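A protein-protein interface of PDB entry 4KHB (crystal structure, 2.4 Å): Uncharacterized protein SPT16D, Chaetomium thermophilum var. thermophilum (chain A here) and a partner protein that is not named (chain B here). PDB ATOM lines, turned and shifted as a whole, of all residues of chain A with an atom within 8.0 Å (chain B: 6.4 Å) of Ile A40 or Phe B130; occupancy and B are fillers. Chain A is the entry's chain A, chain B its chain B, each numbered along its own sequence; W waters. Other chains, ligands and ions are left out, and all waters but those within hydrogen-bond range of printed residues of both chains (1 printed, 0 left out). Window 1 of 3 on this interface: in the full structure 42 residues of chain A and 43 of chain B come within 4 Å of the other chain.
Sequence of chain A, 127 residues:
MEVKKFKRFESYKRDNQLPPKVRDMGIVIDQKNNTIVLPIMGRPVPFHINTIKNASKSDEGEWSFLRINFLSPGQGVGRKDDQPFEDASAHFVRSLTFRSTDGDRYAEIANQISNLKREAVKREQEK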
ATOM      1  N   MET A  25      16.110 -20.456   6.811  1.00  0.00           N
ATOM      2  CA  MET A  25      17.146 -21.298   7.409  1.00  0.00           C
ATOM      3  C   MET A  25      18.319 -20.481   7.941  1.00  0.00           C
ATOM      4  O   MET A  25      19.468 -20.915   7.868  1.00  0.00           O
ATOM      5  CB  MET A  25      17.629 -22.375   6.426  1.00  0.00           C
ATOM      6  CG  MET A  25      16.988 -23.736   6.648  1.00  0.00           C
ATOM      7  SD  MET A  25      17.318 -24.919   5.330  1.00  0.00           S
ATOM      8  CE  MET A  25      15.670 -25.065   4.642  1.00  0.00           C
ATOM      9  N   GLY A  26      18.026 -19.306   8.487  1.00  0.00           N
ATOM     10  CA  GLY A  26      19.068 -18.478   9.064  1.00  0.00           C
ATOM     11  C   GLY A  26      18.866 -18.284  10.551  1.00  0.00           C
ATOM     12  O   GLY A  26      17.800 -18.589  11.090  1.00  0.00           O
ATOM     13  N   VAL A  37      16.734 -18.531  17.588  1.00  0.00           N
ATOM     14  CA  VAL A  37      16.335 -19.692  16.798  1.00  0.00           C
ATOM     15  C   VAL A  37      17.464 -20.098  15.866  1.00  0.00           C
ATOM     16  O   VAL A  37      17.846 -19.343  14.972  1.00  0.00           O
ATOM     17  CB  VAL A  37      15.059 -19.420  15.973  1.00  0.00           C
ATOM     18  CG1 VAL A  37      14.646 -20.673  15.217  1.00  0.00           C
ATOM     19  CG2 VAL A  37      13.932 -18.938  16.869  1.00  0.00           C
ATOM     20  N   LEU A  38      18.001 -21.294  16.083  1.00  0.00           N
ATOM     21  CA  LEU A  38      19.160 -21.745  15.330  1.00  0.00           C
ATOM     22  C   LEU A  38      18.771 -22.791  14.292  1.00  0.00           C
ATOM     23  O   LEU A  38      18.016 -23.719  14.584  1.00  0.00           O
ATOM     24  CB  LEU A  38      20.228 -22.287  16.282  1.00  0.00           C
ATOM     25  CG  LEU A  38      20.542 -21.331  17.436  1.00  0.00           C
ATOM     26  CD1 LEU A  38      21.524 -21.926  18.428  1.00  0.00           C
ATOM     27  CD2 LEU A  38      21.069 -20.017  16.888  1.00  0.00           C
ATOM     28  N   PRO A  39      19.294 -22.637  13.068  1.00  0.00           N
ATOM     29  CA  PRO A  39      18.989 -23.551  11.965  1.00  0.00           C
ATOM     30  C   PRO A  39      19.846 -24.812  12.032  1.00  0.00           C
ATOM     31  O   PRO A  39      21.054 -24.758  11.796  1.00  0.00           O
ATOM     32  CB  PRO A  39      19.343 -22.723  10.727  1.00  0.00           C
ATOM     33  CG  PRO A  39      20.424 -21.795  11.195  1.00  0.00           C
ATOM     34  CD  PRO A  39      20.120 -21.491  12.638  1.00  0.00           C
ATOM     35  N   ILE A  40      19.221 -25.936  12.367  1.00  0.00           N
ATOM     36  CA  ILE A  40      19.945 -27.196  12.476  1.00  0.00           C
ATOM     37  C   ILE A  40      19.339 -28.265  11.572  1.00  0.00           C
ATOM     38  O   ILE A  40      18.256 -28.792  11.849  1.00  0.00           O
ATOM     39  CB  ILE A  40      19.979 -27.705  13.935  1.00  0.00           C
ATOM     40  CG1 ILE A  40      20.590 -26.641  14.853  1.00  0.00           C
ATOM     41  CG2 ILE A  40      20.772 -29.000  14.042  1.00  0.00           C
ATOM     42  CD1 ILE A  40      20.557 -26.996  16.332  1.00  0.00           C
ATOM     43  N   MET A  41      20.054 -28.570  10.490  1.00  0.00           N
ATOM     44  CA  MET A  41      19.671 -29.617   9.543  1.00  0.00           C
ATOM     45  C   MET A  41      18.272 -29.422   8.966  1.00  0.00           C
ATOM     46  O   MET A  41      17.507 -30.379   8.819  1.00  0.00           O
ATOM     47  CB  MET A  41      19.809 -30.998  10.187  1.00  0.00           C
ATOM     48  CG  MET A  41      21.241 -31.327  10.587  1.00  0.00           C
ATOM     49  SD  MET A  41      22.332 -31.512   9.161  1.00  0.00           S
ATOM     50  CE  MET A  41      23.932 -31.131   9.883  1.00  0.00           C
ATOM     51  N   GLY A  42      17.949 -28.175   8.636  1.00  0.00           N
ATOM     52  CA  GLY A  42      16.693 -27.869   7.981  1.00  0.00           C
ATOM     53  C   GLY A  42      15.589 -27.567   8.967  1.00  0.00           C
ATOM     54  O   GLY A  42      14.423 -27.426   8.590  1.00  0.00           O
ATOM     55  N   ARG A  43      15.955 -27.468  10.239  1.00  0.00           N
ATOM     56  CA  ARG A  43      14.974 -27.274  11.292  1.00  0.00           C
ATOM     57  C   ARG A  43      15.339 -26.070  12.145  1.00  0.00           C
ATOM     58  O   ARG A  43      16.468 -25.956  12.627  1.00  0.00           O
ATOM     59  CB  ARG A  43      14.871 -28.535  12.151  1.00  0.00           C
ATOM     60  CG  ARG A  43      13.933 -28.414  13.343  1.00  0.00           C
ATOM     61  CD  ARG A  43      13.663 -29.776  13.965  1.00  0.00           C
ATOM     62  NE  ARG A  43      13.177 -30.730  12.971  1.00  0.00           N
ATOM     63  CZ  ARG A  43      11.930 -30.769  12.514  1.00  0.00           C
ATOM     64  NH1 ARG A  43      11.026 -29.907  12.962  1.00  0.00           N
ATOM     65  NH2 ARG A  43      11.583 -31.672  11.607  1.00  0.00           N
ATOM     66  N   PRO A  44      14.373 -25.164  12.333  1.00  0.00           N
ATOM     67  CA  PRO A  44      14.529 -24.001  13.210  1.00  0.00           C
ATOM     68  C   PRO A  44      14.427 -24.402  14.672  1.00  0.00           C
ATOM     69  O   PRO A  44      13.340 -24.757  15.133  1.00  0.00           O
ATOM     70  CB  PRO A  44      13.344 -23.114  12.825  1.00  0.00           C
ATOM     71  CG  PRO A  44      12.318 -24.063  12.276  1.00  0.00           C
ATOM     72  CD  PRO A  44      13.078 -25.175  11.628  1.00  0.00           C
ATOM     73  N   VAL A  45      15.539 -24.339  15.397  1.00  0.00           N
ATOM     74  CA  VAL A  45      15.555 -24.803  16.778  1.00  0.00           C
ATOM     75  C   VAL A  45      15.688 -23.646  17.760  1.00  0.00           C
ATOM     76  O   VAL A  45      16.677 -22.913  17.737  1.00  0.00           O
ATOM     77  CB  VAL A  45      16.685 -25.815  17.020  1.00  0.00           C
ATOM     78  CG1 VAL A  45      16.623 -26.341  18.445  1.00  0.00           C
ATOM     79  CG2 VAL A  45      16.591 -26.959  16.025  1.00  0.00           C
ATOM     80  N   PRO A  46      14.682 -23.486  18.632  1.00  0.00           N
ATOM     81  CA  PRO A  46      14.664 -22.420  19.639  1.00  0.00           C
ATOM     82  C   PRO A  46      15.585 -22.724  20.811  1.00  0.00           C
ATOM     83  O   PRO A  46      15.649 -23.870  21.255  1.00  0.00           O
ATOM     84  CB  PRO A  46      13.204 -22.412  20.125  1.00  0.00           C
ATOM     85  CG  PRO A  46      12.439 -23.255  19.143  1.00  0.00           C
ATOM     86  CD  PRO A  46      13.419 -24.244  18.611  1.00  0.00           C
ATOM     87  N   PHE A  47      16.289 -21.707  21.296  1.00  0.00           N
ATOM     88  CA  PHE A  47      17.020 -21.807  22.553  1.00  0.00           C
ATOM     89  C   PHE A  47      16.739 -20.559  23.379  1.00  0.00           C
ATOM     90  O   PHE A  47      16.978 -19.435  22.931  1.00  0.00           O
ATOM     91  CB  PHE A  47      18.520 -21.972  22.304  1.00  0.00           C
ATOM     92  CG  PHE A  47      18.904 -23.324  21.765  1.00  0.00           C
ATOM     93  CD1 PHE A  47      19.085 -24.401  22.626  1.00  0.00           C
ATOM     94  CD2 PHE A  47      19.084 -23.521  20.403  1.00  0.00           C
ATOM     95  CE1 PHE A  47      19.443 -25.651  22.137  1.00  0.00           C
ATOM     96  CE2 PHE A  47      19.441 -24.768  19.907  1.00  0.00           C
ATOM     97  CZ  PHE A  47      19.619 -25.833  20.775  1.00  0.00           C
ATOM     98  N   PHE A  70      26.494 -22.555  26.176  1.00  0.00           N
ATOM     99  CA  PHE A  70      25.295 -22.730  26.982  1.00  0.00           C
ATOM    100  C   PHE A  70      25.622 -22.995  28.450  1.00  0.00           C
ATOM    101  O   PHE A  70      26.737 -23.399  28.781  1.00  0.00           O
ATOM    102  CB  PHE A  70      24.474 -23.885  26.412  1.00  0.00           C
ATOM    103  CG  PHE A  70      23.952 -23.628  25.028  1.00  0.00           C
ATOM    104  CD1 PHE A  70      22.739 -22.989  24.846  1.00  0.00           C
ATOM    105  CD2 PHE A  70      24.671 -24.026  23.909  1.00  0.00           C
ATOM    106  CE1 PHE A  70      22.244 -22.748  23.578  1.00  0.00           C
ATOM    107  CE2 PHE A  70      24.185 -23.787  22.634  1.00  0.00           C
ATOM    108  CZ  PHE A  70      22.970 -23.148  22.469  1.00  0.00           C
ATOM    109  N   PHE A  92      23.422 -32.275  28.269  1.00  0.00           N
ATOM    110  CA  PHE A  92      23.277 -30.862  27.931  1.00  0.00           C
ATOM    111  C   PHE A  92      23.906 -30.561  26.575  1.00  0.00           C
ATOM    112  O   PHE A  92      24.886 -31.201  26.185  1.00  0.00           O
ATOM    113  CB  PHE A  92      23.942 -29.982  29.000  1.00  0.00           C
ATOM    114  CG  PHE A  92      23.137 -29.828  30.265  1.00  0.00           C
ATOM    115  CD1 PHE A  92      23.045 -30.862  31.188  1.00  0.00           C
ATOM    116  CD2 PHE A  92      22.497 -28.625  30.541  1.00  0.00           C
ATOM    117  CE1 PHE A  92      22.307 -30.704  32.357  1.00  0.00           C
ATOM    118  CE2 PHE A  92      21.764 -28.459  31.705  1.00  0.00           C
ATOM    119  CZ  PHE A  92      21.669 -29.500  32.613  1.00  0.00           C
ATOM    120  N   VAL A  93      23.344 -29.593  25.858  1.00  0.00           N
ATOM    121  CA  VAL A  93      24.048 -28.990  24.736  1.00  0.00           C
ATOM    122  C   VAL A  93      24.978 -27.962  25.364  1.00  0.00           C
ATOM    123  O   VAL A  93      24.510 -27.055  26.055  1.00  0.00           O
ATOM    124  CB  VAL A  93      23.078 -28.297  23.749  1.00  0.00           C
ATOM    125  CG1 VAL A  93      23.835 -27.712  22.567  1.00  0.00           C
ATOM    126  CG2 VAL A  93      22.014 -29.269  23.270  1.00  0.00           C
ATOM    127  N   SER A  95      27.739 -26.274  23.585  1.00  0.00           N
ATOM    128  CA  SER A  95      27.998 -25.211  22.620  1.00  0.00           C
ATOM    129  C   SER A  95      27.756 -25.662  21.183  1.00  0.00           C
ATOM    130  O   SER A  95      27.731 -26.860  20.890  1.00  0.00           O
ATOM    131  CB  SER A  95      29.435 -24.702  22.757  1.00  0.00           C
ATOM    132  OG  SER A  95      30.363 -25.679  22.315  1.00  0.00           O
ATOM    133  N   LEU A  96      27.571 -24.687  20.297  1.00  0.00           N
ATOM    134  CA  LEU A  96      27.562 -24.933  18.858  1.00  0.00           C
ATOM    135  C   LEU A  96      28.196 -23.757  18.118  1.00  0.00           C
ATOM    136  O   LEU A  96      28.125 -22.611  18.577  1.00  0.00           O
ATOM    137  CB  LEU A  96      26.150 -25.234  18.342  1.00  0.00           C
ATOM    138  CG  LEU A  96      24.944 -24.495  18.912  1.00  0.00           C
ATOM    139  CD1 LEU A  96      24.853 -23.105  18.329  1.00  0.00           C
ATOM    140  CD2 LEU A  96      23.671 -25.284  18.642  1.00  0.00           C
ATOM    141  N   PHE A  98      28.711 -21.703  14.327  1.00  0.00           N
ATOM    142  CA  PHE A  98      28.334 -21.455  12.943  1.00  0.00           C
ATOM    143  C   PHE A  98      29.423 -20.644  12.260  1.00  0.00           C
ATOM    144  O   PHE A  98      30.224 -19.979  12.925  1.00  0.00           O
ATOM    145  CB  PHE A  98      27.011 -20.690  12.848  1.00  0.00           C
ATOM    146  CG  PHE A  98      25.814 -21.461  13.319  1.00  0.00           C
ATOM    147  CD1 PHE A  98      25.393 -21.389  14.638  1.00  0.00           C
ATOM    148  CD2 PHE A  98      25.087 -22.239  12.427  1.00  0.00           C
ATOM    149  CE1 PHE A  98      24.280 -22.092  15.063  1.00  0.00           C
ATOM    150  CE2 PHE A  98      23.974 -22.945  12.843  1.00  0.00           C
ATOM    151  CZ  PHE A  98      23.569 -22.872  14.165  1.00  0.00           C
ATOM    152  N   LEU B  17      17.314 -30.529   1.943  1.00  0.00           N
ATOM    153  CA  LEU B  17      17.724 -29.128   2.052  1.00  0.00           C
ATOM    154  C   LEU B  17      18.189 -28.574   0.715  1.00  0.00           C
ATOM    155  O   LEU B  17      19.092 -27.735   0.660  1.00  0.00           O
ATOM    156  CB  LEU B  17      18.800 -28.921   3.131  1.00  0.00           C
ATOM    157  CG  LEU B  17      18.547 -29.553   4.501  1.00  0.00           C
ATOM    158  CD1 LEU B  17      19.495 -28.992   5.552  1.00  0.00           C
ATOM    159  CD2 LEU B  17      17.109 -29.364   4.916  1.00  0.00           C
ATOM    160  N   GLN B  74      15.031 -36.362   3.578  1.00  0.00           N
ATOM    161  CA  GLN B  74      14.185 -35.265   4.030  1.00  0.00           C
ATOM    162  C   GLN B  74      13.459 -34.563   2.886  1.00  0.00           C
ATOM    163  O   GLN B  74      14.088 -34.000   1.987  1.00  0.00           O
ATOM    164  CB  GLN B  74      15.015 -34.260   4.840  1.00  0.00           C
ATOM    165  CG  GLN B  74      15.420 -34.759   6.221  1.00  0.00           C
ATOM    166  CD  GLN B  74      16.478 -33.892   6.873  1.00  0.00           C
ATOM    167  OE1 GLN B  74      17.655 -34.252   6.918  1.00  0.00           O
ATOM    168  NE2 GLN B  74      16.065 -32.732   7.371  1.00  0.00           N
ATOM    169  N   HIS B 103       8.058 -31.846  17.506  1.00  0.00           N
ATOM    170  CA  HIS B 103       9.332 -31.443  18.080  1.00  0.00           C
ATOM    171  C   HIS B 103       9.123 -30.497  19.260  1.00  0.00           C
ATOM    172  O   HIS B 103       8.105 -29.801  19.333  1.00  0.00           O
ATOM    173  CB  HIS B 103      10.226 -30.816  17.009  1.00  0.00           C
ATOM    174  CG  HIS B 103      10.804 -31.813  16.052  1.00  0.00           C
ATOM    175  ND1 HIS B 103      10.033 -32.528  15.162  1.00  0.00           N
ATOM    176  CD2 HIS B 103      12.080 -32.220  15.857  1.00  0.00           C
ATOM    177  CE1 HIS B 103      10.810 -33.329  14.454  1.00  0.00           C
ATOM    178  NE2 HIS B 103      12.057 -33.161  14.856  1.00  0.00           N
ATOM    179  N   LEU B 120      21.743 -38.923  15.325  1.00  0.00           N
ATOM    180  CA  LEU B 120      21.918 -38.543  16.717  1.00  0.00           C
ATOM    181  C   LEU B 120      20.810 -37.561  17.074  1.00  0.00           C
ATOM    182  O   LEU B 120      20.735 -36.465  16.507  1.00  0.00           O
ATOM    183  CB  LEU B 120      23.294 -37.907  16.935  1.00  0.00           C
ATOM    184  CG  LEU B 120      23.559 -37.319  18.321  1.00  0.00           C
ATOM    185  CD1 LEU B 120      23.286 -38.355  19.392  1.00  0.00           C
ATOM    186  CD2 LEU B 120      24.989 -36.812  18.443  1.00  0.00           C
ATOM    187  N   THR B 121      19.948 -37.953  18.008  1.00  0.00           N
ATOM    188  CA  THR B 121      18.794 -37.141  18.374  1.00  0.00           C
ATOM    189  C   THR B 121      18.981 -36.559  19.769  1.00  0.00           C
ATOM    190  O   THR B 121      19.416 -37.260  20.684  1.00  0.00           O
ATOM    191  CB  THR B 121      17.501 -37.986  18.359  1.00  0.00           C
ATOM    192  OG1 THR B 121      17.269 -38.497  17.038  1.00  0.00           O
ATOM    193  CG2 THR B 121      16.302 -37.154  18.789  1.00  0.00           C
ATOM    194  N   PHE B 122      18.654 -35.278  19.930  1.00  0.00           N
ATOM    195  CA  PHE B 122      18.605 -34.672  21.254  1.00  0.00           C
ATOM    196  C   PHE B 122      17.153 -34.485  21.680  1.00  0.00           C
ATOM    197  O   PHE B 122      16.430 -33.656  21.117  1.00  0.00           O
ATOM    198  CB  PHE B 122      19.359 -33.341  21.288  1.00  0.00           C
ATOM    199  CG  PHE B 122      19.596 -32.820  22.677  1.00  0.00           C
ATOM    200  CD1 PHE B 122      20.613 -33.347  23.462  1.00  0.00           C
ATOM    201  CD2 PHE B 122      18.803 -31.806  23.197  1.00  0.00           C
ATOM    202  CE1 PHE B 122      20.834 -32.873  24.744  1.00  0.00           C
ATOM    203  CE2 PHE B 122      19.018 -31.326  24.477  1.00  0.00           C
ATOM    204  CZ  PHE B 122      20.036 -31.861  25.251  1.00  0.00           C
ATOM    205  N   ASN B 123      16.736 -35.257  22.679  1.00  0.00           N
ATOM    206  CA  ASN B 123      15.349 -35.260  23.120  1.00  0.00           C
ATOM    207  C   ASN B 123      15.143 -34.407  24.369  1.00  0.00           C
ATOM    208  O   ASN B 123      15.936 -34.471  25.312  1.00  0.00           O
ATOM    209  CB  ASN B 123      14.872 -36.696  23.383  1.00  0.00           C
ATOM    210  CG  ASN B 123      14.592 -37.467  22.102  1.00  0.00           C
ATOM    211  OD1 ASN B 123      13.855 -37.001  21.235  1.00  0.00           O
ATOM    212  ND2 ASN B 123      15.170 -38.657  21.985  1.00  0.00           N
ATOM    213  N   ARG B 127      10.757 -35.646  23.462  1.00  0.00           N
ATOM    214  CA  ARG B 127      10.420 -35.054  22.173  1.00  0.00           C
ATOM    215  C   ARG B 127      11.663 -34.403  21.581  1.00  0.00           C
ATOM    216  O   ARG B 127      12.360 -33.645  22.258  1.00  0.00           O
ATOM    217  CB  ARG B 127       9.274 -34.043  22.309  1.00  0.00           C
ATOM    218  CG  ARG B 127       7.959 -34.666  22.760  1.00  0.00           C
ATOM    219  CD  ARG B 127       6.816 -33.664  22.777  1.00  0.00           C
ATOM    220  NE  ARG B 127       5.602 -34.247  23.345  1.00  0.00           N
ATOM    221  CZ  ARG B 127       4.627 -33.543  23.913  1.00  0.00           C
ATOM    222  NH1 ARG B 127       4.711 -32.221  23.988  1.00  0.00           N
ATOM    223  NH2 ARG B 127       3.565 -34.162  24.407  1.00  0.00           N
ATOM    224  N   PRO B 128      11.941 -34.699  20.304  1.00  0.00           N
ATOM    225  CA  PRO B 128      13.165 -34.239  19.641  1.00  0.00           C
ATOM    226  C   PRO B 128      13.224 -32.725  19.495  1.00  0.00           C
ATOM    227  O   PRO B 128      12.264 -32.114  19.029  1.00  0.00           O
ATOM    228  CB  PRO B 128      13.087 -34.904  18.259  1.00  0.00           C
ATOM    229  CG  PRO B 128      11.627 -35.158  18.040  1.00  0.00           C
ATOM    230  CD  PRO B 128      11.080 -35.483  19.400  1.00  0.00           C
ATOM    231  N   ALA B 129      14.336 -32.128  19.903  1.00  0.00           N
ATOM    232  CA  ALA B 129      14.574 -30.718  19.634  1.00  0.00           C
ATOM    233  C   ALA B 129      15.239 -30.587  18.271  1.00  0.00           C
ATOM    234  O   ALA B 129      14.897 -29.703  17.480  1.00  0.00           O
ATOM    235  CB  ALA B 129      15.449 -30.103  20.716  1.00  0.00           C
ATOM    236  N   PHE B 130      16.196 -31.477  18.010  1.00  0.00           N
ATOM    237  CA  PHE B 130      16.872 -31.539  16.715  1.00  0.00           C
ATOM    238  C   PHE B 130      17.504 -32.905  16.436  1.00  0.00           C
ATOM    239  O   PHE B 130      17.701 -33.709  17.350  1.00  0.00           O
ATOM    240  CB  PHE B 130      17.909 -30.422  16.584  1.00  0.00           C
ATOM    241  CG  PHE B 130      18.997 -30.473  17.619  1.00  0.00           C
ATOM    242  CD1 PHE B 130      20.198 -31.117  17.354  1.00  0.00           C
ATOM    243  CD2 PHE B 130      18.826 -29.854  18.850  1.00  0.00           C
ATOM    244  CE1 PHE B 130      21.206 -31.153  18.303  1.00  0.00           C
ATOM    245  CE2 PHE B 130      19.826 -29.886  19.803  1.00  0.00           C
ATOM    246  CZ  PHE B 130      21.020 -30.536  19.529  1.00  0.00           C
ATOM    247  N   GLU B 131      17.821 -33.160  15.169  1.00  0.00           N
ATOM    248  CA  GLU B 131      18.406 -34.433  14.758  1.00  0.00           C
ATOM    249  C   GLU B 131      19.630 -34.197  13.878  1.00  0.00           C
ATOM    250  O   GLU B 131      19.633 -33.291  13.040  1.00  0.00           O
ATOM    251  CB  GLU B 131      17.378 -35.265  13.985  1.00  0.00           C
ATOM    252  CG  GLU B 131      16.121 -35.607  14.767  1.00  0.00           C
ATOM    253  CD  GLU B 131      14.937 -34.761  14.346  1.00  0.00           C
ATOM    254  OE1 GLU B 131      15.161 -33.702  13.723  1.00  0.00           O
ATOM    255  OE2 GLU B 131      13.788 -35.155  14.633  1.00  0.00           O
ATOM    256  N   ILE B 132      20.668 -35.006  14.074  1.00  0.00           N
ATOM    257  CA  ILE B 132      21.866 -34.937  13.240  1.00  0.00           C
ATOM    258  C   ILE B 132      22.139 -36.285  12.576  1.00  0.00           C
ATOM    259  O   ILE B 132      22.482 -37.258  13.251  1.00  0.00           O
ATOM    260  CB  ILE B 132      23.098 -34.522  14.058  1.00  0.00           C
ATOM    261  CG1 ILE B 132      22.867 -33.147  14.683  1.00  0.00           C
ATOM    262  CG2 ILE B 132      24.332 -34.456  13.171  1.00  0.00           C
ATOM    263  CD1 ILE B 132      23.377 -33.022  16.094  1.00  0.00           C
ATOM    264  N   LYS B 170      24.249 -30.801   4.173  1.00  0.00           N
ATOM    265  CA  LYS B 170      23.113 -30.239   4.903  1.00  0.00           C
ATOM    266  C   LYS B 170      23.556 -29.208   5.935  1.00  0.00           C
ATOM    267  O   LYS B 170      22.792 -28.313   6.296  1.00  0.00           O
ATOM    268  CB  LYS B 170      22.282 -31.336   5.577  1.00  0.00           C
ATOM    269  CG  LYS B 170      21.556 -32.264   4.617  1.00  0.00           C
ATOM    270  CD  LYS B 170      20.690 -33.261   5.378  1.00  0.00           C
ATOM    271  CE  LYS B 170      19.862 -34.105   4.424  1.00  0.00           C
ATOM    272  NZ  LYS B 170      19.020 -35.109   5.129  1.00  0.00           N
ATOM    273  N   LEU B 178      26.600 -24.835   9.941  1.00  0.00           N
ATOM    274  CA  LEU B 178      26.905 -25.477  11.213  1.00  0.00           C
ATOM    275  C   LEU B 178      28.309 -26.066  11.162  1.00  0.00           C
ATOM    276  O   LEU B 178      28.652 -26.804  10.232  1.00  0.00           O
ATOM    277  CB  LEU B 178      25.870 -26.557  11.541  1.00  0.00           C
ATOM    278  CG  LEU B 178      25.998 -27.222  12.912  1.00  0.00           C
ATOM    279  CD1 LEU B 178      25.892 -26.180  14.010  1.00  0.00           C
ATOM    280  CD2 LEU B 178      24.920 -28.283  13.094  1.00  0.00           C
ATOM    281  N   ILE B 181      29.024 -29.081  17.169  1.00  0.00           N
ATOM    282  CA  ILE B 181      28.137 -29.136  18.331  1.00  0.00           C
ATOM    283  C   ILE B 181      28.836 -29.915  19.439  1.00  0.00           C
ATOM    284  O   ILE B 181      29.432 -30.966  19.190  1.00  0.00           O
ATOM    285  CB  ILE B 181      26.793 -29.823  18.017  1.00  0.00           C
ATOM    286  CG1 ILE B 181      26.166 -29.218  16.759  1.00  0.00           C
ATOM    287  CG2 ILE B 181      25.834 -29.688  19.196  1.00  0.00           C
ATOM    288  CD1 ILE B 181      24.779 -29.735  16.451  1.00  0.00           C
ATOM    289  N   PHE B 183      28.370 -31.711  23.302  1.00  0.00           N
ATOM    290  CA  PHE B 183      27.396 -32.209  24.261  1.00  0.00           C
ATOM    291  C   PHE B 183      28.094 -32.532  25.573  1.00  0.00           C
ATOM    292  O   PHE B 183      29.220 -33.039  25.575  1.00  0.00           O
ATOM    293  CB  PHE B 183      26.719 -33.473  23.726  1.00  0.00           C
ATOM    294  CG  PHE B 183      25.894 -33.248  22.491  1.00  0.00           C
ATOM    295  CD1 PHE B 183      24.565 -32.865  22.592  1.00  0.00           C
ATOM    296  CD2 PHE B 183      26.445 -33.427  21.230  1.00  0.00           C
ATOM    297  CE1 PHE B 183      23.799 -32.657  21.458  1.00  0.00           C
ATOM    298  CE2 PHE B 183      25.688 -33.222  20.090  1.00  0.00           C
ATOM    299  CZ  PHE B 183      24.362 -32.835  20.204  1.00  0.00           C
HETATM  300  O   HOH W   1      17.101 -30.864  13.173  1.00  0.00           O
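Hydrophobic or aromatic side chains of chain A within 4 Å of the printed part of chain B: Ile A40, Met A41, Val A45, Val A93 and Phe A98. Of the 17 printed residues of chain B, 11 touch a printed residue of chain A. Printed residues of chain B that touch a printed residue of chain A: Leu B17, Gln B74, His B103, Phe B122, Ala B129, Phe B130, Glu B131, Lys B170, Leu B178, Ile B181 and Phe B183. Hydrophobic or aromatic side chains of chain B within 4 Å of the printed part of chain A: Leu B17, His B103, Phe B122, Phe B130, Leu B178, Ile B181 and Phe B183. Among the printed residues, 15 pairs touch across the chains. Among the printed residues, Asp or Glu carboxylates within 4 Å of a Lys or Arg side-chain nitrogen of the other chain: Arg A43 with Glu B131.
O of Met A41 is in hydrogen-bond range of NE2 of Gln B74. NE of Arg A43 lies within hydrogen-bond range of NE2 of His B103. The guanidinium group (NE) of Arg A43 is in salt-bridge range of the side-chain carboxylate (OE1) of Glu B131, at 3.7 Å.
The backbone carbonyl oxygen of Val A45 lies within hydrogen-bond range of the backbone NH of Leu A38, at 2.7 Å. The side-chain amino group of Lys B170 sits at hydrogen-bond distance from the side-chain amide oxygen of Gln B74, 2.4 Å away. NE2 of His B103 lies within hydrogen-bond range of OE2 of Glu B131. The backbone carbonyl oxygen (O) of Phe B122 sits at hydrogen-bond distance from the backbone NH (N) of Ala B129, 2.9 Å away. The backbone NH of Phe B122 sits at hydrogen-bond distance from the backbone carbonyl oxygen of Phe B130.
Ile A40 touches Phe B130. Leu B17 touches Met A41. Glu B131 touches Met A41. Lys B170 touches Met A41 (CB to SD, 3.6 Å). Arg A43 touches Ala B129. CG2 of Val A45 touches O of Ala B129, 3.5 Å away. Phe B130 touches Val A45 (CB to CG2, 3.7 Å). Phe B183 touches Phe A92 (CA to O, 3.3 Å). Val A93 touches Phe B122. Ile B181 touches Ser A95 (CA to O, 3.4 Å).
Water W1 bridges the backbone carbonyl oxygen of Ile A40 (2.7 Å) and the backbone NH of Glu B131 (3.1 Å).
Ile A40 touches one residue of chain B. Phe B130 touches two residues of chain A. Ala B129 touches two residues of chain A. Of the printed residues of chain A, Gln B74 touches Met A41. Printed residues of chain A within 4 Å of Ile B181: Ser A95. Of the printed residues of chain B, Arg A43 touches His B103 (3.3 Å), Ala B129 (3.7 Å) and Glu B131 (3.7 Å). Of the printed residues of chain A, Phe B183 touches Phe A92 (3.3 Å). Printed residues of chain A within 4 Å of Glu B131: Met A41 (3.5 Å) and Arg A43 (3.7 Å). Leu B120 touches none of the printed residues of chain A. The nearest residue of chain B that does not touch Ile A40 is Leu B178 (4.3 Å). The nearest printed residue of chain B that does not touch Val A45 is Glu B131 (6.4 Å).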
